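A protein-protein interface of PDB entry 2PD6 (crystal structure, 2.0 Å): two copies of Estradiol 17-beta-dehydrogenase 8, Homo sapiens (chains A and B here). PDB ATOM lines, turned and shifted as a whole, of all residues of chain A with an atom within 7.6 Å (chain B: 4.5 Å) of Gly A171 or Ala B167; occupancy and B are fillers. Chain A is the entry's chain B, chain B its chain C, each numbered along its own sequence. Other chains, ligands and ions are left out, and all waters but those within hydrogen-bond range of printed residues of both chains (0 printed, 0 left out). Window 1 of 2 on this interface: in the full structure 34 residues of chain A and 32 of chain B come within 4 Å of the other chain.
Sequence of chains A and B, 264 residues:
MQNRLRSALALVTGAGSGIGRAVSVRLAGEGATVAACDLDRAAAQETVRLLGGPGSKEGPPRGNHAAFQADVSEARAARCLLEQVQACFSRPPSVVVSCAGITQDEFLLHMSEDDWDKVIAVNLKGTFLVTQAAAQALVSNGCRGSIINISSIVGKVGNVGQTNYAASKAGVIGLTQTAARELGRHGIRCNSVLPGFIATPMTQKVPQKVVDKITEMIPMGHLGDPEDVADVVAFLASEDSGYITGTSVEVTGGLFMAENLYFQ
The backbone carbonyl oxygen of Gly A174 lies within hydrogen-bond range of the side-chain hydroxyl of Thr A178 (3.1 Å).
Among the printed residues, pairs that only touch across the chains: Leu A124 with Trp B116 (3.8 Å), Phe A128 with Trp B116 (3.4 Å), Ala A167 with Gly B171 (3.5 Å), Ala A170 with Ala B170 (3.2 Å), Gly A171 with Ala B167 (3.5 Å), Gly A171 with Gly B171 (3.9 Å), Thr A178 with Thr B163 (3.2 Å) and Thr A178 with Ala B166 (3.4 Å).
Printed residues of chain B within 4 Å of Leu A124: Trp B116. Thr A127 touches none of the printed residues of chain B. Of the printed residues of chain B, Phe A128 touches Trp B116 (3.4 Å). Gly A171 touches just these residues of chain B: Ala B167 and Gly B171. Of chain A, only Gly A171 comes within 4 Å of Ala B167. The nearest residue of chain B that does not touch Gly A171 is Ala B170 (4.1 Å). The nearest printed residue of chain A that does not touch Gly B171 is Ala A170 (4.2 Å).
Of the 22 printed residues of chain A, 6 touch a printed residue of chain B. Hydrophobic or aromatic side chains of chain A that line the printed part of chain B: Leu A124, Phe A128, Ala A167 and Ala A170. Along chain A the printed residues that touch a printed residue of chain B span positions 124 to 178. Printed residues of chain B that touch a printed residue of chain A: Trp B116, Thr B163, Ala B166, Ala B167, Ala B170 and Gly B171. Hydrophobic or aromatic side chains of chain B within 4 Å of the printed part of chain A: Trp B116, Ala B166, Ala B167 and Ala B170. Among the printed residues, no Asp or Glu carboxylate lies within 4 Å of a Lys or Arg side-chain nitrogen of the other chain.
Ala A167 touches Gly B171, and with the chains exchanged Gly A171 touches Ala B167. Ala A170 touches its own counterpart, Ala B170. Gly B171 touches its own counterpart, Gly A171. 7 positions are printed for both chains.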
ATOM      1  N   ILE A 120      12.289 -25.020  20.512  1.00  0.00           N
ATOM      2  CA  ILE A 120      12.365 -25.112  21.964  1.00  0.00           C
ATOM      3  C   ILE A 120      11.331 -26.146  22.449  1.00  0.00           C
ATOM      4  O   ILE A 120      11.654 -26.999  23.280  1.00  0.00           O
ATOM      5  CB  ILE A 120      12.169 -23.741  22.650  1.00  0.00           C
ATOM      6  CG1 ILE A 120      13.322 -22.804  22.319  1.00  0.00           C
ATOM      7  CG2 ILE A 120      12.076 -23.885  24.166  1.00  0.00           C
ATOM      8  CD1 ILE A 120      14.685 -23.193  22.866  1.00  0.00           C
ATOM      9  N   ASN A 123      12.552 -29.963  21.187  1.00  0.00           N
ATOM     10  CA  ASN A 123      13.860 -30.439  21.626  1.00  0.00           C
ATOM     11  C   ASN A 123      14.079 -30.346  23.114  1.00  0.00           C
ATOM     12  O   ASN A 123      14.741 -31.214  23.686  1.00  0.00           O
ATOM     13  CB  ASN A 123      14.998 -29.666  20.953  1.00  0.00           C
ATOM     14  CG  ASN A 123      15.039 -29.835  19.445  1.00  0.00           C
ATOM     15  OD1 ASN A 123      14.242 -30.569  18.870  1.00  0.00           O
ATOM     16  ND2 ASN A 123      16.020 -29.186  18.804  1.00  0.00           N
ATOM     17  N   LEU A 124      13.593 -29.270  23.717  1.00  0.00           N
ATOM     18  CA  LEU A 124      13.879 -28.962  25.128  1.00  0.00           C
ATOM     19  C   LEU A 124      12.675 -29.289  26.015  1.00  0.00           C
ATOM     20  O   LEU A 124      12.796 -30.019  26.977  1.00  0.00           O
ATOM     21  CB  LEU A 124      14.274 -27.478  25.299  1.00  0.00           C
ATOM     22  CG  LEU A 124      14.565 -27.059  26.752  1.00  0.00           C
ATOM     23  CD1 LEU A 124      15.639 -27.960  27.338  1.00  0.00           C
ATOM     24  CD2 LEU A 124      14.988 -25.608  26.866  1.00  0.00           C
ATOM     25  N   THR A 127      11.949 -33.142  25.648  1.00  0.00           N
ATOM     26  CA  THR A 127      12.889 -33.923  26.447  1.00  0.00           C
ATOM     27  C   THR A 127      12.637 -33.799  27.965  1.00  0.00           C
ATOM     28  O   THR A 127      12.786 -34.776  28.713  1.00  0.00           O
ATOM     29  CB  THR A 127      14.331 -33.589  26.061  1.00  0.00           C
ATOM     30  OG1 THR A 127      14.555 -34.065  24.733  1.00  0.00           O
ATOM     31  CG2 THR A 127      15.312 -34.289  26.986  1.00  0.00           C
ATOM     32  N   PHE A 128      12.272 -32.615  28.424  1.00  0.00           N
ATOM     33  CA  PHE A 128      11.858 -32.430  29.834  1.00  0.00           C
ATOM     34  C   PHE A 128      10.640 -33.309  30.173  1.00  0.00           C
ATOM     35  O   PHE A 128      10.633 -34.033  31.171  1.00  0.00           O
ATOM     36  CB  PHE A 128      11.506 -30.960  30.107  1.00  0.00           C
ATOM     37  CG  PHE A 128      10.695 -30.761  31.361  1.00  0.00           C
ATOM     38  CD1 PHE A 128      11.284 -30.899  32.603  1.00  0.00           C
ATOM     39  CD2 PHE A 128       9.337 -30.452  31.300  1.00  0.00           C
ATOM     40  CE1 PHE A 128      10.523 -30.754  33.789  1.00  0.00           C
ATOM     41  CE2 PHE A 128       8.593 -30.270  32.471  1.00  0.00           C
ATOM     42  CZ  PHE A 128       9.197 -30.441  33.709  1.00  0.00           C
ATOM     43  N   SER A 151      21.403 -34.851  22.861  1.00  0.00           N
ATOM     44  CA  SER A 151      21.583 -33.422  22.679  1.00  0.00           C
ATOM     45  C   SER A 151      22.362 -33.210  21.358  1.00  0.00           C
ATOM     46  O   SER A 151      21.982 -33.766  20.334  1.00  0.00           O
ATOM     47  CB  SER A 151      22.274 -32.838  23.914  1.00  0.00           C
ATOM     48  OG  SER A 151      22.579 -31.483  23.697  1.00  0.00           O
ATOM     49  N   GLY A 155      25.202 -27.834  21.123  1.00  0.00           N
ATOM     50  CA  GLY A 155      24.817 -27.354  22.463  1.00  0.00           C
ATOM     51  C   GLY A 155      25.995 -26.930  23.343  1.00  0.00           C
ATOM     52  O   GLY A 155      25.813 -26.206  24.313  1.00  0.00           O
ATOM     53  N   TYR A 165      18.280 -24.014  17.952  1.00  0.00           N
ATOM     54  CA  TYR A 165      18.755 -25.373  18.150  1.00  0.00           C
ATOM     55  C   TYR A 165      19.823 -25.410  19.257  1.00  0.00           C
ATOM     56  O   TYR A 165      19.793 -26.248  20.130  1.00  0.00           O
ATOM     57  CB  TYR A 165      19.313 -25.904  16.827  1.00  0.00           C
ATOM     58  CG  TYR A 165      19.710 -27.379  16.811  1.00  0.00           C
ATOM     59  CD1 TYR A 165      18.743 -28.362  16.656  1.00  0.00           C
ATOM     60  CD2 TYR A 165      21.053 -27.775  16.876  1.00  0.00           C
ATOM     61  CE1 TYR A 165      19.076 -29.714  16.612  1.00  0.00           C
ATOM     62  CE2 TYR A 165      21.413 -29.164  16.825  1.00  0.00           C
ATOM     63  CZ  TYR A 165      20.397 -30.120  16.700  1.00  0.00           C
ATOM     64  OH  TYR A 165      20.661 -31.466  16.619  1.00  0.00           O
ATOM     65  N   ALA A 166      20.753 -24.480  19.209  1.00  0.00           N
ATOM     66  CA  ALA A 166      21.852 -24.407  20.190  1.00  0.00           C
ATOM     67  C   ALA A 166      21.314 -24.173  21.593  1.00  0.00           C
ATOM     68  O   ALA A 166      21.711 -24.859  22.537  1.00  0.00           O
ATOM     69  CB  ALA A 166      22.803 -23.308  19.816  1.00  0.00           C
ATOM     70  N   ALA A 167      20.399 -23.230  21.731  1.00  0.00           N
ATOM     71  CA  ALA A 167      19.733 -22.975  23.024  1.00  0.00           C
ATOM     72  C   ALA A 167      19.069 -24.263  23.540  1.00  0.00           C
ATOM     73  O   ALA A 167      19.239 -24.643  24.708  1.00  0.00           O
ATOM     74  CB  ALA A 167      18.727 -21.866  22.883  1.00  0.00           C
ATOM     75  N   SER A 168      18.354 -24.961  22.655  1.00  0.00           N
ATOM     76  CA  SER A 168      17.588 -26.147  23.065  1.00  0.00           C
ATOM     77  C   SER A 168      18.492 -27.294  23.499  1.00  0.00           C
ATOM     78  O   SER A 168      18.173 -28.011  24.469  1.00  0.00           O
ATOM     79  CB  SER A 168      16.642 -26.607  21.946  1.00  0.00           C
ATOM     80  OG  SER A 168      17.372 -27.246  20.889  1.00  0.00           O
ATOM     81  N   LYS A 169      19.637 -27.451  22.831  1.00  0.00           N
ATOM     82  CA  LYS A 169      20.514 -28.579  23.108  1.00  0.00           C
ATOM     83  C   LYS A 169      21.363 -28.307  24.339  1.00  0.00           C
ATOM     84  O   LYS A 169      21.640 -29.213  25.100  1.00  0.00           O
ATOM     85  CB  LYS A 169      21.380 -28.938  21.889  1.00  0.00           C
ATOM     86  CG  LYS A 169      20.583 -29.544  20.657  1.00  0.00           C
ATOM     87  CD  LYS A 169      19.601 -30.689  21.055  1.00  0.00           C
ATOM     88  CE  LYS A 169      19.149 -31.554  19.857  1.00  0.00           C
ATOM     89  NZ  LYS A 169      18.296 -32.766  20.220  1.00  0.00           N
ATOM     90  N   ALA A 170      21.777 -27.057  24.521  1.00  0.00           N
ATOM     91  CA  ALA A 170      22.401 -26.612  25.773  1.00  0.00           C
ATOM     92  C   ALA A 170      21.424 -26.782  26.950  1.00  0.00           C
ATOM     93  O   ALA A 170      21.801 -27.279  27.993  1.00  0.00           O
ATOM     94  CB  ALA A 170      22.861 -25.140  25.645  1.00  0.00           C
ATOM     95  N   GLY A 171      20.182 -26.353  26.770  1.00  0.00           N
ATOM     96  CA  GLY A 171      19.111 -26.595  27.738  1.00  0.00           C
ATOM     97  C   GLY A 171      18.968 -28.066  28.105  1.00  0.00           C
ATOM     98  O   GLY A 171      18.779 -28.389  29.259  1.00  0.00           O
ATOM     99  N   VAL A 172      19.083 -28.964  27.119  1.00  0.00           N
ATOM    100  CA  VAL A 172      18.950 -30.409  27.348  1.00  0.00           C
ATOM    101  C   VAL A 172      20.096 -30.904  28.218  1.00  0.00           C
ATOM    102  O   VAL A 172      19.890 -31.672  29.162  1.00  0.00           O
ATOM    103  CB  VAL A 172      18.829 -31.178  26.008  1.00  0.00           C
ATOM    104  CG1 VAL A 172      19.060 -32.709  26.189  1.00  0.00           C
ATOM    105  CG2 VAL A 172      17.485 -30.867  25.360  1.00  0.00           C
ATOM    106  N   ILE A 173      21.297 -30.404  27.980  1.00  0.00           N
ATOM    107  CA  ILE A 173      22.418 -30.740  28.837  1.00  0.00           C
ATOM    108  C   ILE A 173      22.209 -30.295  30.309  1.00  0.00           C
ATOM    109  O   ILE A 173      22.514 -31.054  31.239  1.00  0.00           O
ATOM    110  CB  ILE A 173      23.759 -30.158  28.295  1.00  0.00           C
ATOM    111  CG1 ILE A 173      24.097 -30.751  26.907  1.00  0.00           C
ATOM    112  CG2 ILE A 173      24.908 -30.473  29.271  1.00  0.00           C
ATOM    113  CD1 ILE A 173      25.071 -29.910  26.068  1.00  0.00           C
ATOM    114  N   GLY A 174      21.740 -29.061  30.506  1.00  0.00           N
ATOM    115  CA  GLY A 174      21.497 -28.539  31.843  1.00  0.00           C
ATOM    116  C   GLY A 174      20.391 -29.304  32.555  1.00  0.00           C
ATOM    117  O   GLY A 174      20.516 -29.631  33.741  1.00  0.00           O
ATOM    118  N   LEU A 175      19.308 -29.561  31.833  1.00  0.00           N
ATOM    119  CA  LEU A 175      18.195 -30.421  32.287  1.00  0.00           C
ATOM    120  C   LEU A 175      18.693 -31.775  32.787  1.00  0.00           C
ATOM    121  O   LEU A 175      18.316 -32.253  33.852  1.00  0.00           O
ATOM    122  CB  LEU A 175      17.230 -30.618  31.121  1.00  0.00           C
ATOM    123  CG  LEU A 175      16.075 -31.620  31.053  1.00  0.00           C
ATOM    124  CD1 LEU A 175      15.364 -31.413  29.708  1.00  0.00           C
ATOM    125  CD2 LEU A 175      16.509 -33.041  31.161  1.00  0.00           C
ATOM    126  N   THR A 176      19.572 -32.376  32.008  1.00  0.00           N
ATOM    127  CA  THR A 176      19.986 -33.753  32.244  1.00  0.00           C
ATOM    128  C   THR A 176      20.896 -33.865  33.459  1.00  0.00           C
ATOM    129  O   THR A 176      20.748 -34.791  34.274  1.00  0.00           O
ATOM    130  CB  THR A 176      20.646 -34.314  30.948  1.00  0.00           C
ATOM    131  OG1 THR A 176      19.649 -34.289  29.933  1.00  0.00           O
ATOM    132  CG2 THR A 176      21.135 -35.741  31.136  1.00  0.00           C
ATOM    133  N   GLN A 177      21.808 -32.909  33.605  1.00  0.00           N
ATOM    134  CA  GLN A 177      22.691 -32.843  34.771  1.00  0.00           C
ATOM    135  C   GLN A 177      21.894 -32.770  36.085  1.00  0.00           C
ATOM    136  O   GLN A 177      22.209 -33.462  37.050  1.00  0.00           O
ATOM    137  CB  GLN A 177      23.583 -31.590  34.719  1.00  0.00           C
ATOM    138  CG  GLN A 177      24.614 -31.521  33.597  1.00  0.00           C
ATOM    139  CD  GLN A 177      25.469 -30.242  33.693  1.00  0.00           C
ATOM    140  OE1 GLN A 177      25.041 -29.150  33.284  1.00  0.00           O
ATOM    141  NE2 GLN A 177      26.655 -30.373  34.307  1.00  0.00           N
ATOM    142  N   THR A 178      20.912 -31.881  36.107  1.00  0.00           N
ATOM    143  CA  THR A 178      20.052 -31.637  37.289  1.00  0.00           C
ATOM    144  C   THR A 178      19.219 -32.885  37.561  1.00  0.00           C
ATOM    145  O   THR A 178      19.141 -33.352  38.690  1.00  0.00           O
ATOM    146  CB  THR A 178      19.081 -30.451  37.054  1.00  0.00           C
ATOM    147  OG1 THR A 178      19.824 -29.262  36.784  1.00  0.00           O
ATOM    148  CG2 THR A 178      18.187 -30.188  38.315  1.00  0.00           C
ATOM    149  N   SER A 192      23.568 -37.545  28.710  1.00  0.00           N
ATOM    150  CA  SER A 192      23.414 -36.912  27.400  1.00  0.00           C
ATOM    151  C   SER A 192      24.396 -37.477  26.403  1.00  0.00           C
ATOM    152  O   SER A 192      25.527 -37.813  26.734  1.00  0.00           O
ATOM    153  CB  SER A 192      23.675 -35.401  27.521  1.00  0.00           C
ATOM    154  OG  SER A 192      22.502 -34.756  27.943  1.00  0.00           O
ATOM    155  N   TRP B 116       7.575 -25.016  34.713  1.00  0.00           N
ATOM    156  CA  TRP B 116       8.578 -25.127  33.637  1.00  0.00           C
ATOM    157  C   TRP B 116       8.457 -23.992  32.601  1.00  0.00           C
ATOM    158  O   TRP B 116       9.443 -23.319  32.278  1.00  0.00           O
ATOM    159  CB  TRP B 116       8.476 -26.502  32.938  1.00  0.00           C
ATOM    160  CG  TRP B 116       9.290 -26.589  31.704  1.00  0.00           C
ATOM    161  CD1 TRP B 116       8.905 -26.244  30.437  1.00  0.00           C
ATOM    162  CD2 TRP B 116      10.644 -27.035  31.596  1.00  0.00           C
ATOM    163  NE1 TRP B 116       9.947 -26.441  29.550  1.00  0.00           N
ATOM    164  CE2 TRP B 116      11.016 -26.943  30.234  1.00  0.00           C
ATOM    165  CE3 TRP B 116      11.574 -27.516  32.509  1.00  0.00           C
ATOM    166  CZ2 TRP B 116      12.281 -27.288  29.783  1.00  0.00           C
ATOM    167  CZ3 TRP B 116      12.845 -27.854  32.048  1.00  0.00           C
ATOM    168  CH2 TRP B 116      13.178 -27.748  30.711  1.00  0.00           C
ATOM    169  N   THR B 163      15.556 -27.754  37.814  1.00  0.00           N
ATOM    170  CA  THR B 163      15.663 -28.306  36.478  1.00  0.00           C
ATOM    171  C   THR B 163      15.269 -27.239  35.460  1.00  0.00           C
ATOM    172  O   THR B 163      15.924 -27.111  34.417  1.00  0.00           O
ATOM    173  CB  THR B 163      14.788 -29.568  36.270  1.00  0.00           C
ATOM    174  OG1 THR B 163      15.337 -30.646  37.024  1.00  0.00           O
ATOM    175  CG2 THR B 163      14.848 -30.007  34.814  1.00  0.00           C
ATOM    176  N   ASN B 164      14.231 -26.467  35.761  1.00  0.00           N
ATOM    177  CA  ASN B 164      13.768 -25.435  34.815  1.00  0.00           C
ATOM    178  C   ASN B 164      14.762 -24.286  34.669  1.00  0.00           C
ATOM    179  O   ASN B 164      15.066 -23.846  33.566  1.00  0.00           O
ATOM    180  CB  ASN B 164      12.367 -24.881  35.160  1.00  0.00           C
ATOM    181  CG  ASN B 164      12.182 -24.563  36.647  1.00  0.00           C
ATOM    182  OD1 ASN B 164      13.100 -24.743  37.472  1.00  0.00           O
ATOM    183  ND2 ASN B 164      10.978 -24.091  36.994  1.00  0.00           N
ATOM    184  N   TYR B 165      15.269 -23.817  35.804  1.00  0.00           N
ATOM    185  CA  TYR B 165      16.201 -22.709  35.838  1.00  0.00           C
ATOM    186  C   TYR B 165      17.500 -23.116  35.165  1.00  0.00           C
ATOM    187  O   TYR B 165      17.996 -22.394  34.308  1.00  0.00           O
ATOM    188  CB  TYR B 165      16.427 -22.300  37.285  1.00  0.00           C
ATOM    189  CG  TYR B 165      17.257 -21.057  37.514  1.00  0.00           C
ATOM    190  CD1 TYR B 165      16.745 -19.773  37.268  1.00  0.00           C
ATOM    191  CD2 TYR B 165      18.550 -21.161  38.039  1.00  0.00           C
ATOM    192  CE1 TYR B 165      17.534 -18.608  37.496  1.00  0.00           C
ATOM    193  CE2 TYR B 165      19.328 -20.009  38.300  1.00  0.00           C
ATOM    194  CZ  TYR B 165      18.829 -18.744  38.017  1.00  0.00           C
ATOM    195  OH  TYR B 165      19.604 -17.631  38.299  1.00  0.00           O
ATOM    196  N   ALA B 166      18.029 -24.279  35.523  1.00  0.00           N
ATOM    197  CA  ALA B 166      19.291 -24.761  34.941  1.00  0.00           C
ATOM    198  C   ALA B 166      19.179 -24.884  33.418  1.00  0.00           C
ATOM    199  O   ALA B 166      20.075 -24.461  32.687  1.00  0.00           O
ATOM    200  CB  ALA B 166      19.691 -26.122  35.568  1.00  0.00           C
ATOM    201  N   ALA B 167      18.096 -25.481  32.933  1.00  0.00           N
ATOM    202  CA  ALA B 167      17.858 -25.559  31.473  1.00  0.00           C
ATOM    203  C   ALA B 167      17.787 -24.153  30.852  1.00  0.00           C
ATOM    204  O   ALA B 167      18.440 -23.871  29.844  1.00  0.00           O
ATOM    205  CB  ALA B 167      16.557 -26.346  31.174  1.00  0.00           C
ATOM    206  N   SER B 168      16.999 -23.255  31.442  1.00  0.00           N
ATOM    207  CA  SER B 168      16.887 -21.895  30.903  1.00  0.00           C
ATOM    208  C   SER B 168      18.250 -21.193  30.871  1.00  0.00           C
ATOM    209  O   SER B 168      18.565 -20.493  29.890  1.00  0.00           O
ATOM    210  CB  SER B 168      15.883 -21.052  31.696  1.00  0.00           C
ATOM    211  OG  SER B 168      16.479 -20.620  32.924  1.00  0.00           O
ATOM    212  N   LYS B 169      19.076 -21.390  31.915  1.00  0.00           N
ATOM    213  CA  LYS B 169      20.353 -20.699  32.014  1.00  0.00           C
ATOM    214  C   LYS B 169      21.429 -21.311  31.111  1.00  0.00           C
ATOM    215  O   LYS B 169      22.249 -20.568  30.577  1.00  0.00           O
ATOM    216  CB  LYS B 169      20.849 -20.611  33.464  1.00  0.00           C
ATOM    217  CG  LYS B 169      20.004 -19.670  34.349  1.00  0.00           C
ATOM    218  CD  LYS B 169      19.758 -18.290  33.732  1.00  0.00           C
ATOM    219  CE  LYS B 169      19.291 -17.254  34.784  1.00  0.00           C
ATOM    220  NZ  LYS B 169      19.023 -15.902  34.193  1.00  0.00           N
ATOM    221  N   ALA B 170      21.424 -22.638  30.936  1.00  0.00           N
ATOM    222  CA  ALA B 170      22.316 -23.310  29.982  1.00  0.00           C
ATOM    223  C   ALA B 170      21.927 -22.837  28.574  1.00  0.00           C
ATOM    224  O   ALA B 170      22.763 -22.500  27.756  1.00  0.00           O
ATOM    225  CB  ALA B 170      22.159 -24.837  30.074  1.00  0.00           C
ATOM    226  N   GLY B 171      20.638 -22.797  28.318  1.00  0.00           N
ATOM    227  CA  GLY B 171      20.121 -22.227  27.075  1.00  0.00           C
ATOM    228  C   GLY B 171      20.665 -20.840  26.732  1.00  0.00           C
ATOM    229  O   GLY B 171      21.063 -20.598  25.611  1.00  0.00           O
